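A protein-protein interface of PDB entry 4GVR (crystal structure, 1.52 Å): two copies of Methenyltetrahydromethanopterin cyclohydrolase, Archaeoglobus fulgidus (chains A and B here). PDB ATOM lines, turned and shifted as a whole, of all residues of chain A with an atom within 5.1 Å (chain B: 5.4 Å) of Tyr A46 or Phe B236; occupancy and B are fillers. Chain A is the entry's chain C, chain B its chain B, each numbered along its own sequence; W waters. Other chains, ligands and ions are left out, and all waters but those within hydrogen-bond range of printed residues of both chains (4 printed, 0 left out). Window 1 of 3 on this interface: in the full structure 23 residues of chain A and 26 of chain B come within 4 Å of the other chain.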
ATOM      1  N   GLY A  44      22.320  13.632 -32.431  1.00  0.00           N
ATOM      2  CA  GLY A  44      22.963  14.388 -31.365  1.00  0.00           C
ATOM      3  C   GLY A  44      22.660  13.763 -29.982  1.00  0.00           C
ATOM      4  O   GLY A  44      22.174  12.595 -29.884  1.00  0.00           O
ATOM      5  N   SER A  45      22.921  14.523 -28.908  1.00  0.00           N
ATOM      6  CA  SER A  45      22.874  13.914 -27.571  1.00  0.00           C
ATOM      7  C   SER A  45      22.875  15.022 -26.533  1.00  0.00           C
ATOM      8  O   SER A  45      23.161  16.187 -26.855  1.00  0.00           O
ATOM      9  CB  SER A  45      24.091  13.001 -27.280  1.00  0.00           C
ATOM     10  OG  SER A  45      25.325  13.752 -27.527  1.00  0.00           O
ATOM     11  N   TYR A  46      22.582  14.679 -25.288  1.00  0.00           N
ATOM     12  CA  TYR A  46      22.660  15.652 -24.227  1.00  0.00           C
ATOM     13  C   TYR A  46      24.054  16.263 -24.139  1.00  0.00           C
ATOM     14  O   TYR A  46      24.189  17.484 -24.055  1.00  0.00           O
ATOM     15  CB  TYR A  46      22.324  14.968 -22.906  1.00  0.00           C
ATOM     16  CG  TYR A  46      20.827  14.801 -22.598  1.00  0.00           C
ATOM     17  CD1 TYR A  46      20.272  13.519 -22.465  1.00  0.00           C
ATOM     18  CD2 TYR A  46      20.008  15.918 -22.498  1.00  0.00           C
ATOM     19  CE1 TYR A  46      18.910  13.373 -22.147  1.00  0.00           C
ATOM     20  CE2 TYR A  46      18.634  15.778 -22.138  1.00  0.00           C
ATOM     21  CZ  TYR A  46      18.129  14.493 -22.068  1.00  0.00           C
ATOM     22  OH  TYR A  46      16.744  14.265 -21.691  1.00  0.00           O
ATOM     23  N   ASP A  47      25.046  15.392 -24.103  1.00  0.00           N
ATOM     24  CA  ASP A  47      26.453  15.916 -24.089  1.00  0.00           C
ATOM     25  C   ASP A  47      26.842  16.766 -25.323  1.00  0.00           C
ATOM     26  O   ASP A  47      27.555  17.789 -25.148  1.00  0.00           O
ATOM     27  CB  ASP A  47      27.431  14.792 -23.838  1.00  0.00           C
ATOM     28  CG  ASP A  47      27.446  14.365 -22.357  1.00  0.00           C
ATOM     29  OD1 ASP A  47      26.972  15.169 -21.462  1.00  0.00           O
ATOM     30  OD2 ASP A  47      27.951  13.231 -22.106  1.00  0.00           O
ATOM     31  N   ALA A  48      26.370  16.402 -26.521  1.00  0.00           N
ATOM     32  CA  ALA A  48      26.669  17.264 -27.689  1.00  0.00           C
ATOM     33  C   ALA A  48      25.994  18.606 -27.443  1.00  0.00           C
ATOM     34  O   ALA A  48      26.539  19.666 -27.804  1.00  0.00           O
ATOM     35  CB  ALA A  48      26.206  16.669 -29.006  1.00  0.00           C
ATOM     36  N   GLY A  49      24.811  18.580 -26.768  1.00  0.00           N
ATOM     37  CA  GLY A  49      24.061  19.835 -26.492  1.00  0.00           C
ATOM     38  C   GLY A  49      24.854  20.759 -25.553  1.00  0.00           C
ATOM     39  O   GLY A  49      24.898  22.001 -25.748  1.00  0.00           O
ATOM     40  N   ILE A  50      25.401  20.164 -24.466  1.00  0.00           N
ATOM     41  CA  ILE A  50      26.231  20.884 -23.491  1.00  0.00           C
ATOM     42  C   ILE A  50      27.469  21.486 -24.226  1.00  0.00           C
ATOM     43  O   ILE A  50      27.772  22.669 -23.980  1.00  0.00           O
ATOM     44  CB  ILE A  50      26.721  19.959 -22.368  1.00  0.00           C
ATOM     45  CG1 ILE A  50      25.497  19.603 -21.430  1.00  0.00           C
ATOM     46  CG2 ILE A  50      27.716  20.640 -21.478  1.00  0.00           C
ATOM     47  CD1 ILE A  50      25.940  18.475 -20.545  1.00  0.00           C
ATOM     48  N   ILE A  65      24.112  19.501 -16.902  1.00  0.00           N
ATOM     49  CA  ILE A  65      22.644  19.071 -16.849  1.00  0.00           C
ATOM     50  C   ILE A  65      22.399  18.350 -15.513  1.00  0.00           C
ATOM     51  O   ILE A  65      23.219  17.496 -15.108  1.00  0.00           O
ATOM     52  CB  ILE A  65      22.209  18.177 -18.018  1.00  0.00           C
ATOM     53  CG1 ILE A  65      22.351  18.995 -19.374  1.00  0.00           C
ATOM     54  CG2 ILE A  65      20.841  17.447 -17.773  1.00  0.00           C
ATOM     55  CD1 ILE A  65      22.039  18.180 -20.620  1.00  0.00           C
ATOM     56  N   PRO A  74       9.316  14.948 -13.792  1.00  0.00           N
ATOM     57  CA  PRO A  74      10.765  15.133 -14.067  1.00  0.00           C
ATOM     58  C   PRO A  74      11.139  15.806 -15.403  1.00  0.00           C
ATOM     59  O   PRO A  74      10.545  15.497 -16.433  1.00  0.00           O
ATOM     60  CB  PRO A  74      11.305  13.701 -14.110  1.00  0.00           C
ATOM     61  CG  PRO A  74      10.090  12.796 -14.316  1.00  0.00           C
ATOM     62  CD  PRO A  74       8.846  13.568 -14.067  1.00  0.00           C
ATOM     63  N   PHE A  75      12.127  16.720 -15.367  1.00  0.00           N
ATOM     64  CA  PHE A  75      12.762  17.263 -16.572  1.00  0.00           C
ATOM     65  C   PHE A  75      14.227  17.293 -16.321  1.00  0.00           C
ATOM     66  O   PHE A  75      14.712  17.398 -15.174  1.00  0.00           O
ATOM     67  CB  PHE A  75      12.291  18.701 -16.835  1.00  0.00           C
ATOM     68  CG  PHE A  75      10.778  18.785 -17.090  1.00  0.00           C
ATOM     69  CD1 PHE A  75       9.837  18.991 -16.043  1.00  0.00           C
ATOM     70  CD2 PHE A  75      10.279  18.568 -18.383  1.00  0.00           C
ATOM     71  CE1 PHE A  75       8.461  19.066 -16.310  1.00  0.00           C
ATOM     72  CE2 PHE A  75       8.876  18.595 -18.630  1.00  0.00           C
ATOM     73  CZ  PHE A  75       7.956  18.832 -17.569  1.00  0.00           C
ATOM     74  N   ALA A  76      14.938  17.214 -17.436  1.00  0.00           N
ATOM     75  CA  ALA A  76      16.382  17.630 -17.448  1.00  0.00           C
ATOM     76  C   ALA A  76      16.481  19.166 -17.466  1.00  0.00           C
ATOM     77  O   ALA A  76      15.678  19.838 -18.163  1.00  0.00           O
ATOM     78  CB  ALA A  76      17.136  17.016 -18.616  1.00  0.00           C
ATOM     79  N   ILE A 174      17.525  17.377 -29.806  1.00  0.00           N
ATOM     80  CA  ILE A 174      17.988  17.448 -28.414  1.00  0.00           C
ATOM     81  C   ILE A 174      19.027  18.570 -28.222  1.00  0.00           C
ATOM     82  O   ILE A 174      19.068  19.301 -27.229  1.00  0.00           O
ATOM     83  CB  ILE A 174      18.468  16.109 -27.791  1.00  0.00           C
ATOM     84  CG1 ILE A 174      18.706  16.287 -26.271  1.00  0.00           C
ATOM     85  CG2 ILE A 174      19.698  15.579 -28.487  1.00  0.00           C
ATOM     86  CD1 ILE A 174      17.400  16.666 -25.509  1.00  0.00           C
ATOM     87  N   VAL A 178      18.670  21.690 -25.623  1.00  0.00           N
ATOM     88  CA  VAL A 178      19.735  21.956 -24.624  1.00  0.00           C
ATOM     89  C   VAL A 178      20.318  23.347 -24.851  1.00  0.00           C
ATOM     90  O   VAL A 178      20.469  24.147 -23.879  1.00  0.00           O
ATOM     91  CB  VAL A 178      20.861  20.883 -24.616  1.00  0.00           C
ATOM     92  CG1 VAL A 178      22.017  21.295 -23.677  1.00  0.00           C
ATOM     93  CG2 VAL A 178      20.255  19.504 -24.285  1.00  0.00           C
ATOM     94  N   ILE A 211      15.041  21.928 -19.835  1.00  0.00           N
ATOM     95  CA  ILE A 211      15.255  21.621 -21.214  1.00  0.00           C
ATOM     96  C   ILE A 211      13.941  21.163 -21.856  1.00  0.00           C
ATOM     97  O   ILE A 211      13.297  20.211 -21.371  1.00  0.00           O
ATOM     98  CB  ILE A 211      16.327  20.518 -21.326  1.00  0.00           C
ATOM     99  CG1 ILE A 211      17.727  21.037 -20.836  1.00  0.00           C
ATOM    100  CG2 ILE A 211      16.434  19.987 -22.763  1.00  0.00           C
ATOM    101  CD1 ILE A 211      18.682  19.964 -20.307  1.00  0.00           C
ATOM    102  N   PRO A 213      11.057  19.391 -23.870  1.00  0.00           N
ATOM    103  CA  PRO A 213      10.793  18.219 -24.725  1.00  0.00           C
ATOM    104  C   PRO A 213      10.968  18.646 -26.215  1.00  0.00           C
ATOM    105  O   PRO A 213      10.820  19.851 -26.570  1.00  0.00           O
ATOM    106  CB  PRO A 213       9.330  17.807 -24.348  1.00  0.00           C
ATOM    107  CG  PRO A 213       9.124  18.469 -23.043  1.00  0.00           C
ATOM    108  CD  PRO A 213       9.905  19.737 -23.006  1.00  0.00           C
ATOM    109  N   TYR B  81      22.152  10.610 -17.064  1.00  0.00           N
ATOM    110  CA  TYR B  81      21.503  10.541 -18.371  1.00  0.00           C
ATOM    111  C   TYR B  81      22.341   9.748 -19.373  1.00  0.00           C
ATOM    112  O   TYR B  81      23.561   9.592 -19.232  1.00  0.00           O
ATOM    113  CB  TYR B  81      21.097  11.945 -18.863  1.00  0.00           C
ATOM    114  CG  TYR B  81      22.270  12.912 -18.940  1.00  0.00           C
ATOM    115  CD1 TYR B  81      22.608  13.753 -17.848  1.00  0.00           C
ATOM    116  CD2 TYR B  81      23.134  12.937 -20.085  1.00  0.00           C
ATOM    117  CE1 TYR B  81      23.680  14.623 -17.894  1.00  0.00           C
ATOM    118  CE2 TYR B  81      24.207  13.818 -20.149  1.00  0.00           C
ATOM    119  CZ  TYR B  81      24.520  14.641 -19.057  1.00  0.00           C
ATOM    120  OH  TYR B  81      25.625  15.488 -19.136  1.00  0.00           O
ATOM    121  N   THR B  82      21.684   9.313 -20.432  1.00  0.00           N
ATOM    122  CA  THR B  82      22.394   8.578 -21.493  1.00  0.00           C
ATOM    123  C   THR B  82      21.618   8.732 -22.816  1.00  0.00           C
ATOM    124  O   THR B  82      20.338   8.759 -22.855  1.00  0.00           O
ATOM    125  CB  THR B  82      22.505   7.070 -21.146  1.00  0.00           C
ATOM    126  OG1 THR B  82      23.176   6.352 -22.208  1.00  0.00           O
ATOM    127  CG2 THR B  82      21.078   6.420 -20.838  1.00  0.00           C
ATOM    128  N   ASP B  83      22.382   8.800 -23.903  1.00  0.00           N
ATOM    129  CA  ASP B  83      21.821   8.760 -25.247  1.00  0.00           C
ATOM    130  C   ASP B  83      22.049   7.405 -25.949  1.00  0.00           C
ATOM    131  O   ASP B  83      21.883   7.290 -27.180  1.00  0.00           O
ATOM    132  CB  ASP B  83      22.390   9.926 -26.059  1.00  0.00           C
ATOM    133  CG  ASP B  83      21.727  11.232 -25.658  1.00  0.00           C
ATOM    134  OD1 ASP B  83      22.216  11.860 -24.684  1.00  0.00           O
ATOM    135  OD2 ASP B  83      20.676  11.570 -26.267  1.00  0.00           O
ATOM    136  N   SER B 204      16.657   8.365 -25.657  1.00  0.00           N
ATOM    137  CA  SER B 204      17.515   8.746 -24.534  1.00  0.00           C
ATOM    138  C   SER B 204      16.727   8.694 -23.231  1.00  0.00           C
ATOM    139  O   SER B 204      15.453   8.584 -23.195  1.00  0.00           O
ATOM    140  CB  SER B 204      18.025  10.184 -24.690  1.00  0.00           C
ATOM    141  OG  SER B 204      16.945  11.089 -24.868  1.00  0.00           O
ATOM    142  N   GLY B 205      17.440   8.806 -22.111  1.00  0.00           N
ATOM    143  CA  GLY B 205      16.711   8.918 -20.835  1.00  0.00           C
ATOM    144  C   GLY B 205      17.563   9.637 -19.794  1.00  0.00           C
ATOM    145  O   GLY B 205      18.818   9.570 -19.803  1.00  0.00           O
ATOM    146  N   ALA B 206      16.881  10.315 -18.875  1.00  0.00           N
ATOM    147  CA  ALA B 206      17.516  11.120 -17.815  1.00  0.00           C
ATOM    148  C   ALA B 206      16.784  10.798 -16.525  1.00  0.00           C
ATOM    149  O   ALA B 206      15.588  10.760 -16.530  1.00  0.00           O
ATOM    150  CB  ALA B 206      17.376  12.604 -18.112  1.00  0.00           C
ATOM    151  N   GLY B 207      17.528  10.609 -15.458  1.00  0.00           N
ATOM    152  CA  GLY B 207      16.886  10.201 -14.194  1.00  0.00           C
ATOM    153  C   GLY B 207      17.512  10.781 -12.952  1.00  0.00           C
ATOM    154  O   GLY B 207      18.701  11.213 -12.987  1.00  0.00           O
ATOM    155  N   SER B 234      12.711   9.240 -10.490  1.00  0.00           N
ATOM    156  CA  SER B 234      11.988   9.948 -11.560  1.00  0.00           C
ATOM    157  C   SER B 234      12.784   9.895 -12.857  1.00  0.00           C
ATOM    158  O   SER B 234      14.031  10.125 -12.841  1.00  0.00           O
ATOM    159  CB  SER B 234      11.659  11.411 -11.179  1.00  0.00           C
ATOM    160  OG  SER B 234      11.275  11.536  -9.828  1.00  0.00           O
ATOM    161  N   VAL B 235      12.081   9.634 -13.979  1.00  0.00           N
ATOM    162  CA  VAL B 235      12.815   9.466 -15.245  1.00  0.00           C
ATOM    163  C   VAL B 235      12.129  10.268 -16.327  1.00  0.00           C
ATOM    164  O   VAL B 235      10.931  10.166 -16.517  1.00  0.00           O
ATOM    165  CB  VAL B 235      12.857   7.983 -15.688  1.00  0.00           C
ATOM    166  CG1 VAL B 235      13.699   7.807 -16.964  1.00  0.00           C
ATOM    167  CG2 VAL B 235      13.473   7.097 -14.615  1.00  0.00           C
ATOM    168  N   PHE B 236      12.911  11.067 -17.043  1.00  0.00           N
ATOM    169  CA  PHE B 236      12.444  11.721 -18.279  1.00  0.00           C
ATOM    170  C   PHE B 236      13.055  10.934 -19.459  1.00  0.00           C
ATOM    171  O   PHE B 236      14.263  10.724 -19.476  1.00  0.00           O
ATOM    172  CB  PHE B 236      12.886  13.197 -18.308  1.00  0.00           C
ATOM    173  CG  PHE B 236      12.426  13.935 -19.537  1.00  0.00           C
ATOM    174  CD1 PHE B 236      11.229  14.684 -19.550  1.00  0.00           C
ATOM    175  CD2 PHE B 236      13.160  13.837 -20.712  1.00  0.00           C
ATOM    176  CE1 PHE B 236      10.796  15.325 -20.722  1.00  0.00           C
ATOM    177  CE2 PHE B 236      12.754  14.494 -21.877  1.00  0.00           C
ATOM    178  CZ  PHE B 236      11.592  15.239 -21.890  1.00  0.00           C
ATOM    179  N   LEU B 237      12.208  10.494 -20.382  1.00  0.00           N
ATOM    180  CA  LEU B 237      12.529   9.575 -21.463  1.00  0.00           C
ATOM    181  C   LEU B 237      12.075  10.174 -22.753  1.00  0.00           C
ATOM    182  O   LEU B 237      11.069  10.882 -22.782  1.00  0.00           O
ATOM    183  CB  LEU B 237      11.735   8.239 -21.308  1.00  0.00           C
ATOM    184  CG  LEU B 237      12.010   7.345 -20.135  1.00  0.00           C
ATOM    185  CD1 LEU B 237      10.762   6.543 -19.724  1.00  0.00           C
ATOM    186  CD2 LEU B 237      13.195   6.445 -20.499  1.00  0.00           C
ATOM    187  N   THR B 238      12.811   9.870 -23.833  1.00  0.00           N
ATOM    188  CA  THR B 238      12.435  10.292 -25.177  1.00  0.00           C
ATOM    189  C   THR B 238      12.329   9.064 -26.067  1.00  0.00           C
ATOM    190  O   THR B 238      13.250   8.217 -26.037  1.00  0.00           O
ATOM    191  CB  THR B 238      13.466  11.265 -25.782  1.00  0.00           C
ATOM    192  OG1 THR B 238      13.574  12.392 -24.904  1.00  0.00           O
ATOM    193  CG2 THR B 238      12.961  11.757 -27.108  1.00  0.00           C
ATOM    194  N   ALA B 286       8.166  10.756 -17.299  1.00  0.00           N
ATOM    195  CA  ALA B 286       7.572  11.630 -18.322  1.00  0.00           C
ATOM    196  C   ALA B 286       8.178  11.129 -19.641  1.00  0.00           C
ATOM    197  O   ALA B 286       9.376  10.884 -19.692  1.00  0.00           O
ATOM    198  CB  ALA B 286       7.896  13.067 -18.014  1.00  0.00           C
ATOM    199  N   ASN B 288       8.591  11.666 -23.690  1.00  0.00           N
ATOM    200  CA  ASN B 288       8.411  12.636 -24.717  1.00  0.00           C
ATOM    201  C   ASN B 288       8.392  11.827 -26.003  1.00  0.00           C
ATOM    202  O   ASN B 288       9.394  11.146 -26.377  1.00  0.00           O
ATOM    203  CB  ASN B 288       9.650  13.557 -24.734  1.00  0.00           C
ATOM    204  CG  ASN B 288       9.754  14.497 -25.952  1.00  0.00           C
ATOM    205  OD1 ASN B 288       8.793  14.840 -26.670  1.00  0.00           O
ATOM    206  ND2 ASN B 288      10.952  14.970 -26.130  1.00  0.00           N
ATOM    207  N   THR B 295       4.216  14.969 -24.403  1.00  0.00           N
ATOM    208  CA  THR B 295       4.961  14.337 -23.339  1.00  0.00           C
ATOM    209  C   THR B 295       3.977  13.774 -22.256  1.00  0.00           C
ATOM    210  O   THR B 295       3.171  14.499 -21.536  1.00  0.00           O
ATOM    211  CB  THR B 295       6.024  15.299 -22.743  1.00  0.00           C
ATOM    212  OG1 THR B 295       7.079  15.522 -23.711  1.00  0.00           O
ATOM    213  CG2 THR B 295       6.703  14.720 -21.505  1.00  0.00           C
HETATM  214  O   HOH W   1      15.580  12.001 -22.670  1.00  0.00           O
HETATM  215  O   HOH W   2      25.609  10.706 -21.778  1.00  0.00           O
HETATM  216  O   HOH W   3      26.191  17.532 -17.262  1.00  0.00           O
HETATM  217  O   HOH W   4      24.833  12.453 -23.739  1.00  0.00           O
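Ser A45 touches Asp B83 (CB to CG, 3.4 Å).
Tyr A46 touches Tyr B81 (CB to CE2, 3.5 Å).
Tyr A46 touches Ala B206 (OH to CB, 3.996 Å).
Phe B236 touches Tyr A46.
Ile A50 touches Tyr B81 (CD1 to OH, 3.3 Å).
CE1 of Tyr B81 touches CB of Ile A65 (3.8 Å).
Pro A74 touches Ser B234.
Phe B236 touches Pro A74.
CB of Ala B286 touches O of Pro A74 (3.9 Å).
Asn B288 touches Pro A213 (ND2 to CA, 3.5 Å).
The side-chain carboxylate of Asp A47 lies within hydrogen-bond range of the side-chain hydroxyl of Tyr B81 (2.7 Å).
The side-chain carboxylate (OD1) of Asp B83 lies within hydrogen-bond range of the backbone NH (N) of Tyr A46 (2.9 Å).
No position is printed for both chains.
Of the 14 pairs that touch across the chains among the printed residues, none has its exchanged pair printed and touching as well.
O of Phe B236 is in hydrogen-bond range of N of Ala B206, 2.7 Å away.
The backbone carbonyl oxygen (O) of Val B235 lies within hydrogen-bond range of the backbone NH (N) of Ala B286, at 2.9 Å.
N of Leu B237 sits at hydrogen-bond distance from O of Ala B286 (2.9 Å).
O of Leu B237 lies within hydrogen-bond range of N of Asn B288.
The side-chain amide oxygen (OD1) of Asn B288 sits close to the side-chain hydroxyl (OG1) of Thr B295, 3.5 Å away.
OG of Ser A45 sits at hydrogen-bond distance from N of Ala A48, at 3.0 Å.
Water W1 lies within hydrogen-bond range of OH of Tyr A46, OG of Ser B204 and OG1 of Thr B238.
Water W3 bridges the side-chain hydroxyl (OH) of Tyr B81 (2.8 Å) and the backbone NH (N) of Ile A65 (2.9 Å).
Water W4 bridges OD1 of Asp B83 and N of Asp A47.
Water W2 lies within hydrogen-bond range of the backbone carbonyl oxygen of Tyr B81 and the side-chain carboxylate of Asp A47.
Hydrophobic or aromatic side chains of chain B within 4 Å of the printed part of chain A: Tyr B81, Ala B206, Phe B236 and Ala B286.
Printed residues of chain A that touch a printed residue of chain B: Ser A45, Tyr A46, Asp A47, Ile A50, Ile A65, Pro A74 and Pro A213.
Among the printed residues, no Asp or Glu carboxylate lies within 4 Å of a Lys or Arg side-chain nitrogen of the other chain.
Gly A44 touches none of the printed residues of chain B.
Of the printed residues of chain B, Tyr A46 touches Tyr B81 (3.5 Å), Asp B83 (2.9 Å), Ala B206 (3.996 Å) and Phe B236 (3.7 Å).
Of the printed residues of chain B, Asp A47 touches Tyr B81.
Printed residues of chain A within 4 Å of Tyr B81: Tyr A46 (3.5 Å), Asp A47 (2.7 Å), Ile A50 (3.3 Å) and Ile A65 (3.8 Å).
Of the printed residues of chain A, Ala B206 touches Tyr A46.
Phe B236 touches two residues of chain A.
Thr B238 touches none of the printed residues of chain A.
Of the printed residues of chain A, Thr B295 touches Pro A213.
The nearest printed residue of chain A that does not touch Ala B286 is Phe A75 (5.6 Å).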
